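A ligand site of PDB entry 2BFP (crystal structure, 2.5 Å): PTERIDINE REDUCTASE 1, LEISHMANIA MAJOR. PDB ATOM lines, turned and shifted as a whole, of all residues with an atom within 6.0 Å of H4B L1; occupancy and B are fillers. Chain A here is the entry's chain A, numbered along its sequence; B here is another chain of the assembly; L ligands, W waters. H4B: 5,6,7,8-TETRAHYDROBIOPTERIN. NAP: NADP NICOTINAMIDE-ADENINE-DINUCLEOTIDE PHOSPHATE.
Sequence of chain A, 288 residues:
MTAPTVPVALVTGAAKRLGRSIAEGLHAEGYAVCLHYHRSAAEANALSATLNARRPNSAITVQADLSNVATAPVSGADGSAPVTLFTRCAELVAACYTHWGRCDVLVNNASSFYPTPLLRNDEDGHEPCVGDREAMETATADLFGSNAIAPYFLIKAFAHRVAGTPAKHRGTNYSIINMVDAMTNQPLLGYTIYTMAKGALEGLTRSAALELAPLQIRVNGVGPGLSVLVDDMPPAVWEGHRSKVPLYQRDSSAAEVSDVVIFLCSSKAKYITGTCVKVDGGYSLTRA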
ATOM      1  N   ARG A  17      -3.386  12.950 -29.910  1.00  0.00           N
ATOM      2  CA  ARG A  17      -3.261  11.810 -29.011  1.00  0.00           C
ATOM      3  C   ARG A  17      -4.463  10.858 -28.980  1.00  0.00           C
ATOM      4  O   ARG A  17      -4.924  10.431 -30.048  1.00  0.00           O
ATOM      5  CB  ARG A  17      -2.809  12.292 -27.624  1.00  0.00           C
ATOM      6  CG  ARG A  17      -1.385  12.860 -27.660  1.00  0.00           C
ATOM      7  CD  ARG A  17      -1.030  13.836 -26.568  1.00  0.00           C
ATOM      8  NE  ARG A  17      -1.181  13.221 -25.256  1.00  0.00           N
ATOM      9  CZ  ARG A  17      -0.351  12.317 -24.753  1.00  0.00           C
ATOM     10  NH1 ARG A  17       0.711  11.926 -25.449  1.00  0.00           N
ATOM     11  NH2 ARG A  17      -0.585  11.781 -23.562  1.00  0.00           N
ATOM     12  N   ASN A 109     -13.570  13.141 -23.633  1.00  0.00           N
ATOM     13  CA  ASN A 109     -12.133  12.854 -23.643  1.00  0.00           C
ATOM     14  C   ASN A 109     -11.277  14.037 -23.202  1.00  0.00           C
ATOM     15  O   ASN A 109     -10.238  13.832 -22.590  1.00  0.00           O
ATOM     16  CB  ASN A 109     -11.718  12.352 -25.039  1.00  0.00           C
ATOM     17  CG  ASN A 109     -10.203  12.236 -25.212  1.00  0.00           C
ATOM     18  OD1 ASN A 109      -9.596  11.246 -24.829  1.00  0.00           O
ATOM     19  ND2 ASN A 109      -9.613  13.234 -25.830  1.00  0.00           N
ATOM     20  N   ALA A 110     -11.716  15.254 -23.509  1.00  0.00           N
ATOM     21  CA  ALA A 110     -10.949  16.460 -23.156  1.00  0.00           C
ATOM     22  C   ALA A 110     -10.670  16.441 -21.673  1.00  0.00           C
ATOM     23  O   ALA A 110     -11.549  16.092 -20.882  1.00  0.00           O
ATOM     24  CB  ALA A 110     -11.680  17.730 -23.546  1.00  0.00           C
ATOM     25  N   SER A 111      -9.452  16.834 -21.293  1.00  0.00           N
ATOM     26  CA  SER A 111      -9.045  16.757 -19.903  1.00  0.00           C
ATOM     27  C   SER A 111      -7.753  17.492 -19.591  1.00  0.00           C
ATOM     28  O   SER A 111      -6.730  17.332 -20.274  1.00  0.00           O
ATOM     29  CB  SER A 111      -8.876  15.268 -19.529  1.00  0.00           C
ATOM     30  OG  SER A 111      -7.923  15.052 -18.496  1.00  0.00           O
ATOM     31  N   SER A 112      -7.806  18.340 -18.575  1.00  0.00           N
ATOM     32  CA  SER A 112      -6.585  19.000 -18.150  1.00  0.00           C
ATOM     33  C   SER A 112      -5.932  18.124 -17.068  1.00  0.00           C
ATOM     34  O   SER A 112      -6.609  17.427 -16.301  1.00  0.00           O
ATOM     35  CB  SER A 112      -6.806  20.454 -17.712  1.00  0.00           C
ATOM     36  OG  SER A 112      -7.817  20.586 -16.749  1.00  0.00           O
ATOM     37  N   PHE A 113      -4.601  18.155 -17.032  1.00  0.00           N
ATOM     38  CA  PHE A 113      -3.829  17.319 -16.140  1.00  0.00           C
ATOM     39  C   PHE A 113      -2.514  17.988 -15.719  1.00  0.00           C
ATOM     40  O   PHE A 113      -1.608  18.164 -16.548  1.00  0.00           O
ATOM     41  CB  PHE A 113      -3.558  15.998 -16.875  1.00  0.00           C
ATOM     42  CG  PHE A 113      -2.632  15.057 -16.155  1.00  0.00           C
ATOM     43  CD1 PHE A 113      -3.051  14.355 -15.021  1.00  0.00           C
ATOM     44  CD2 PHE A 113      -1.338  14.843 -16.641  1.00  0.00           C
ATOM     45  CE1 PHE A 113      -2.201  13.478 -14.379  1.00  0.00           C
ATOM     46  CE2 PHE A 113      -0.473  13.980 -15.984  1.00  0.00           C
ATOM     47  CZ  PHE A 113      -0.906  13.296 -14.858  1.00  0.00           C
ATOM     48  N   ASN A 147     -12.615  17.582 -16.791  1.00  0.00           N
ATOM     49  CA  ASN A 147     -12.744  16.199 -16.397  1.00  0.00           C
ATOM     50  C   ASN A 147     -14.092  15.789 -15.831  1.00  0.00           C
ATOM     51  O   ASN A 147     -14.404  14.593 -15.859  1.00  0.00           O
ATOM     52  CB  ASN A 147     -11.668  15.835 -15.344  1.00  0.00           C
ATOM     53  CG  ASN A 147     -10.263  15.908 -15.892  1.00  0.00           C
ATOM     54  OD1 ASN A 147      -9.883  15.111 -16.746  1.00  0.00           O
ATOM     55  ND2 ASN A 147      -9.505  16.893 -15.427  1.00  0.00           N
ATOM     56  N   ASP A 181      -9.575   6.940 -15.593  1.00  0.00           N
ATOM     57  CA  ASP A 181      -8.153   6.717 -15.381  1.00  0.00           C
ATOM     58  C   ASP A 181      -7.981   5.463 -14.547  1.00  0.00           C
ATOM     59  O   ASP A 181      -8.363   5.445 -13.388  1.00  0.00           O
ATOM     60  CB  ASP A 181      -7.542   7.909 -14.655  1.00  0.00           C
ATOM     61  CG  ASP A 181      -6.036   7.785 -14.435  1.00  0.00           C
ATOM     62  OD1 ASP A 181      -5.466   6.670 -14.418  1.00  0.00           O
ATOM     63  OD2 ASP A 181      -5.317   8.787 -14.239  1.00  0.00           O
ATOM     64  N   LEU A 188      -1.570   9.543  -8.035  1.00  0.00           N
ATOM     65  CA  LEU A 188      -0.323  10.118  -8.480  1.00  0.00           C
ATOM     66  C   LEU A 188      -0.042  11.211  -7.454  1.00  0.00           C
ATOM     67  O   LEU A 188      -0.888  12.096  -7.215  1.00  0.00           O
ATOM     68  CB  LEU A 188      -0.550  10.699  -9.861  1.00  0.00           C
ATOM     69  CG  LEU A 188       0.614  10.905 -10.824  1.00  0.00           C
ATOM     70  CD1 LEU A 188       1.572   9.705 -10.897  1.00  0.00           C
ATOM     71  CD2 LEU A 188       0.038  11.240 -12.200  1.00  0.00           C
ATOM     72  N   TYR A 194      -7.090  16.683  -9.843  1.00  0.00           N
ATOM     73  CA  TYR A 194      -7.266  15.864 -11.035  1.00  0.00           C
ATOM     74  C   TYR A 194      -7.857  14.504 -10.666  1.00  0.00           C
ATOM     75  O   TYR A 194      -8.802  14.029 -11.297  1.00  0.00           O
ATOM     76  CB  TYR A 194      -5.935  15.648 -11.760  1.00  0.00           C
ATOM     77  CG  TYR A 194      -5.978  14.483 -12.735  1.00  0.00           C
ATOM     78  CD1 TYR A 194      -6.468  14.644 -14.021  1.00  0.00           C
ATOM     79  CD2 TYR A 194      -5.546  13.214 -12.342  1.00  0.00           C
ATOM     80  CE1 TYR A 194      -6.515  13.569 -14.911  1.00  0.00           C
ATOM     81  CE2 TYR A 194      -5.586  12.141 -13.213  1.00  0.00           C
ATOM     82  CZ  TYR A 194      -6.064  12.315 -14.494  1.00  0.00           C
ATOM     83  OH  TYR A 194      -6.108  11.241 -15.375  1.00  0.00           O
ATOM     84  N   LYS A 198     -11.535  12.853 -11.684  1.00  0.00           N
ATOM     85  CA  LYS A 198     -11.765  11.566 -12.323  1.00  0.00           C
ATOM     86  C   LYS A 198     -12.714  10.721 -11.475  1.00  0.00           C
ATOM     87  O   LYS A 198     -13.586  10.021 -12.004  1.00  0.00           O
ATOM     88  CB  LYS A 198     -10.472  10.827 -12.632  1.00  0.00           C
ATOM     89  CG  LYS A 198      -9.630  11.471 -13.734  1.00  0.00           C
ATOM     90  CD  LYS A 198     -10.372  11.552 -15.074  1.00  0.00           C
ATOM     91  CE  LYS A 198      -9.361  11.870 -16.169  1.00  0.00           C
ATOM     92  NZ  LYS A 198      -9.983  12.076 -17.486  1.00  0.00           N
ATOM     93  N   GLY A 225      -4.021   3.456 -18.514  1.00  0.00           N
ATOM     94  CA  GLY A 225      -3.030   3.368 -17.449  1.00  0.00           C
ATOM     95  C   GLY A 225      -1.987   4.359 -17.890  1.00  0.00           C
ATOM     96  O   GLY A 225      -2.015   5.524 -17.492  1.00  0.00           O
ATOM     97  N   LEU A 226      -1.061   3.899 -18.729  1.00  0.00           N
ATOM     98  CA  LEU A 226      -0.039   4.783 -19.297  1.00  0.00           C
ATOM     99  C   LEU A 226      -0.190   4.680 -20.799  1.00  0.00           C
ATOM    100  O   LEU A 226      -0.042   3.598 -21.374  1.00  0.00           O
ATOM    101  CB  LEU A 226       1.366   4.359 -18.877  1.00  0.00           C
ATOM    102  CG  LEU A 226       1.681   4.448 -17.369  1.00  0.00           C
ATOM    103  CD1 LEU A 226       3.156   4.136 -17.088  1.00  0.00           C
ATOM    104  CD2 LEU A 226       1.296   5.804 -16.758  1.00  0.00           C
ATOM    105  N   SER A 227      -0.609   5.781 -21.432  1.00  0.00           N
ATOM    106  CA  SER A 227      -0.771   5.783 -22.892  1.00  0.00           C
ATOM    107  C   SER A 227      -0.017   6.902 -23.567  1.00  0.00           C
ATOM    108  O   SER A 227      -0.169   8.045 -23.162  1.00  0.00           O
ATOM    109  CB  SER A 227      -2.231   5.852 -23.282  1.00  0.00           C
ATOM    110  OG  SER A 227      -2.858   4.665 -22.871  1.00  0.00           O
ATOM    111  N   LEU A 229       2.758   7.936 -23.401  1.00  0.00           N
ATOM    112  CA  LEU A 229       3.388   8.646 -22.298  1.00  0.00           C
ATOM    113  C   LEU A 229       4.192   9.829 -22.808  1.00  0.00           C
ATOM    114  O   LEU A 229       4.967   9.677 -23.744  1.00  0.00           O
ATOM    115  CB  LEU A 229       4.235   7.678 -21.480  1.00  0.00           C
ATOM    116  CG  LEU A 229       4.604   8.047 -20.045  1.00  0.00           C
ATOM    117  CD1 LEU A 229       3.347   8.245 -19.183  1.00  0.00           C
ATOM    118  CD2 LEU A 229       5.576   7.026 -19.438  1.00  0.00           C
ATOM    119  N   VAL A 230       3.940  11.008 -22.263  1.00  0.00           N
ATOM    120  CA  VAL A 230       4.691  12.185 -22.687  1.00  0.00           C
ATOM    121  C   VAL A 230       6.144  11.980 -22.252  1.00  0.00           C
ATOM    122  O   VAL A 230       6.412  11.682 -21.090  1.00  0.00           O
ATOM    123  CB  VAL A 230       4.123  13.492 -22.086  1.00  0.00           C
ATOM    124  CG1 VAL A 230       5.014  14.676 -22.478  1.00  0.00           C
ATOM    125  CG2 VAL A 230       2.663  13.695 -22.540  1.00  0.00           C
ATOM    126  N   ARG B 287       1.742   2.176  -6.175  1.00  0.00           N
ATOM    127  CA  ARG B 287       1.845   1.571  -7.504  1.00  0.00           C
ATOM    128  C   ARG B 287       3.329   1.325  -7.722  1.00  0.00           C
ATOM    129  O   ARG B 287       4.157   1.926  -7.043  1.00  0.00           O
ATOM    130  CB  ARG B 287       1.290   2.520  -8.569  1.00  0.00           C
ATOM    131  CG  ARG B 287       1.946   3.880  -8.629  1.00  0.00           C
ATOM    132  CD  ARG B 287       1.543   4.695  -9.850  1.00  0.00           C
ATOM    133  NE  ARG B 287       0.272   5.431  -9.677  1.00  0.00           N
ATOM    134  CZ  ARG B 287      -0.281   6.180 -10.627  1.00  0.00           C
ATOM    135  NH1 ARG B 287       0.298   6.274 -11.818  1.00  0.00           N
ATOM    136  NH2 ARG B 287      -1.410   6.814 -10.407  1.00  0.00           N
HETATM  137  N1  H4B L   1      -4.602  12.983 -18.343  1.00  0.00           N
HETATM  138  C2  H4B L   1      -4.451  13.829 -19.399  1.00  0.00           C
HETATM  139  N2  H4B L   1      -5.381  14.704 -19.720  1.00  0.00           N
HETATM  140  N3  H4B L   1      -3.317  13.756 -20.115  1.00  0.00           N
HETATM  141  C4  H4B L   1      -2.270  12.865 -19.857  1.00  0.00           C
HETATM  142  O4  H4B L   1      -1.283  12.886 -20.607  1.00  0.00           O
HETATM  143  C4A H4B L   1      -2.493  11.999 -18.739  1.00  0.00           C
HETATM  144  C8A H4B L   1      -3.644  12.064 -17.983  1.00  0.00           C
HETATM  145  N5  H4B L   1      -1.428  11.046 -18.414  1.00  0.00           N
HETATM  146  N8  H4B L   1      -3.850  11.349 -16.884  1.00  0.00           N
HETATM  147  C6  H4B L   1      -1.799  10.016 -17.368  1.00  0.00           C
HETATM  148  C7  H4B L   1      -2.758  10.567 -16.324  1.00  0.00           C
HETATM  149  C9  H4B L   1      -0.552   9.255 -16.848  1.00  0.00           C
HETATM  150  O9  H4B L   1       0.192   8.679 -17.925  1.00  0.00           O
HETATM  151  C10 H4B L   1       0.407   9.990 -15.893  1.00  0.00           C
HETATM  152  C11 H4B L   1       1.391  10.917 -16.497  1.00  0.00           C
HETATM  153  O10 H4B L   1       1.120   8.940 -15.239  1.00  0.00           O
HETATM  154  PA  NAP L   2      -4.351  14.985 -23.404  1.00  0.00           P
HETATM  155  O1A NAP L   2      -3.633  15.237 -22.136  1.00  0.00           O
HETATM  156  O2A NAP L   2      -3.377  14.876 -24.572  1.00  0.00           O
HETATM  157  O5B NAP L   2      -5.438  16.116 -23.650  1.00  0.00           O
HETATM  158  C5B NAP L   2      -6.559  15.918 -24.451  1.00  0.00           C
HETATM  159  C4B NAP L   2      -7.207  17.267 -24.754  1.00  0.00           C
HETATM  160  O4B NAP L   2      -8.016  17.802 -23.711  1.00  0.00           O
HETATM  161  C3B NAP L   2      -6.190  18.369 -24.996  1.00  0.00           C
HETATM  162  O3B NAP L   2      -5.580  18.226 -26.250  1.00  0.00           O
HETATM  163  C2B NAP L   2      -7.034  19.636 -24.869  1.00  0.00           C
HETATM  164  O2B NAP L   2      -7.442  20.175 -26.111  1.00  0.00           O
HETATM  165  C1B NAP L   2      -8.251  19.143 -24.081  1.00  0.00           C
HETATM  166  N9A NAP L   2      -8.451  20.003 -22.915  1.00  0.00           N
HETATM  167  C8A NAP L   2      -7.680  20.152 -21.803  1.00  0.00           C
HETATM  168  N7A NAP L   2      -8.237  21.071 -20.976  1.00  0.00           N
HETATM  169  C5A NAP L   2      -9.353  21.531 -21.586  1.00  0.00           C
HETATM  170  C6A NAP L   2     -10.306  22.471 -21.229  1.00  0.00           C
HETATM  171  N6A NAP L   2     -10.110  23.329 -20.233  1.00  0.00           N
HETATM  172  N1A NAP L   2     -11.338  22.718 -22.098  1.00  0.00           N
HETATM  173  C2A NAP L   2     -11.440  22.058 -23.298  1.00  0.00           C
HETATM  174  N3A NAP L   2     -10.502  21.119 -23.639  1.00  0.00           N
HETATM  175  C4A NAP L   2      -9.490  20.867 -22.795  1.00  0.00           C
HETATM  176  O3  NAP L   2      -5.190  13.635 -23.180  1.00  0.00           O
HETATM  177  PN  NAP L   2      -4.695  12.135 -23.552  1.00  0.00           P
HETATM  178  O1N NAP L   2      -3.399  11.848 -22.895  1.00  0.00           O
HETATM  179  O2N NAP L   2      -4.893  11.912 -24.997  1.00  0.00           O
HETATM  180  O5D NAP L   2      -5.837  11.316 -22.754  1.00  0.00           O
HETATM  181  C5D NAP L   2      -7.169  11.321 -23.183  1.00  0.00           C
HETATM  182  C4D NAP L   2      -8.060  10.943 -22.006  1.00  0.00           C
HETATM  183  O4D NAP L   2      -7.575   9.754 -21.407  1.00  0.00           O
HETATM  184  C3D NAP L   2      -8.063  12.024 -20.937  1.00  0.00           C
HETATM  185  O3D NAP L   2      -9.349  12.086 -20.367  1.00  0.00           O
HETATM  186  C2D NAP L   2      -7.094  11.464 -19.912  1.00  0.00           C
HETATM  187  O2D NAP L   2      -7.371  11.907 -18.612  1.00  0.00           O
HETATM  188  C1D NAP L   2      -7.338   9.972 -20.030  1.00  0.00           C
HETATM  189  N1N NAP L   2      -6.108   9.310 -19.594  1.00  0.00           N
HETATM  190  C2N NAP L   2      -4.941   9.443 -20.310  1.00  0.00           C
HETATM  191  C3N NAP L   2      -3.783   8.816 -19.864  1.00  0.00           C
HETATM  192  C7N NAP L   2      -2.521   8.767 -20.663  1.00  0.00           C
HETATM  193  O7N NAP L   2      -1.493   7.952 -20.162  1.00  0.00           O
HETATM  194  N7N NAP L   2      -2.360   9.433 -21.804  1.00  0.00           N
HETATM  195  C4N NAP L   2      -3.855   8.061 -18.700  1.00  0.00           C
HETATM  196  C5N NAP L   2      -5.032   7.938 -17.982  1.00  0.00           C
HETATM  197  C6N NAP L   2      -6.176   8.574 -18.446  1.00  0.00           C
HETATM  198  P2B NAP L   2      -6.677  21.364 -26.888  1.00  0.00           P
HETATM  199  O1X NAP L   2      -7.380  21.690 -28.149  1.00  0.00           O
HETATM  200  O2X NAP L   2      -6.568  22.640 -26.061  1.00  0.00           O
HETATM  201  O3X NAP L   2      -5.254  20.854 -27.162  1.00  0.00           O
HETATM  202  O   HOH W   1      -2.567   6.958 -15.234  1.00  0.00           O
HETATM  203  O   HOH W   2       1.271  10.835 -20.440  1.00  0.00           O
HETATM  204  O   HOH W   3      -0.758   8.039 -13.550  1.00  0.00           O
HETATM  205  O   HOH W   4      -0.109  15.052 -21.498  1.00  0.00           O
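The guanidinium group of Arg 17 lies within hydrogen-bond range of an oxygen (O4) of H4B L1 (3.2 Å). NE of Arg 17 lies within salt-bridge range of O2A of NAP L2. N8 of H4B L1 lies within hydrogen-bond range of OH of Tyr 194 (2.7 Å). O3D of NAP L2 is in hydrogen-bond range of O of Asn 109, 3.0 Å away. The side-chain hydroxyl (OG) of Ser 111 sits at hydrogen-bond distance from a nitrogen (N2) of H4B L1 (2.8 Å). The side-chain hydroxyl (OG) of Ser 111 is in hydrogen-bond range of an oxygen (O2D) of NAP L2. NZ of Lys 198 sits at hydrogen-bond distance from O2D of NAP L2 (2.8 Å). The backbone carbonyl oxygen (O) of Ser 227 is in hydrogen-bond range of a nitrogen (N7N) of NAP L2, at 2.9 Å. An oxygen (O7N) of NAP L2 is in hydrogen-bond range of the backbone NH (N) of Ser 227, 2.7 Å away. O4B of NAP L2 sits at hydrogen-bond distance from N of Ser 111 (3.0 Å). A nitrogen (N2) of H4B L1 lies within hydrogen-bond range of the backbone carbonyl oxygen of Ser 111 (3.0 Å).
A nitrogen (N3) of H4B L1 is in hydrogen-bond range of an oxygen (O1A) of NAP L2 (2.5 Å).
The side-chain hydroxyl (OG) of Ser 111 lies within hydrogen-bond range of the side-chain amide oxygen (OD1) of Asn 147 (2.6 Å). The side-chain carboxylate (OD2) of Asp 181 lies within hydrogen-bond range of the side-chain hydroxyl (OH) of Tyr 194 (2.8 Å).
Merely in contact with H4B L1: Leu 226 (3.3 Å), Leu 229 (3.4 Å), Phe 113 (3.4 Å), Asp 181 (3.8 Å), Gly 225 (3.9 Å) and Leu 188 (3.9 Å). The nearest printed residue that does not touch H4B L1 is Ser 112 (4.4 Å).
Water W3 bridges an oxygen (O10) of H4B L1 and the guanidinium group of Arg 287 of chain B. Water W2 bridges N of Val 230 (3.2 Å) and O4 of H4B L1 (3.3 Å). Water W1 bridges O of Gly 225 (2.7 Å) and OD1 of Asp 181 (3.0 Å).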
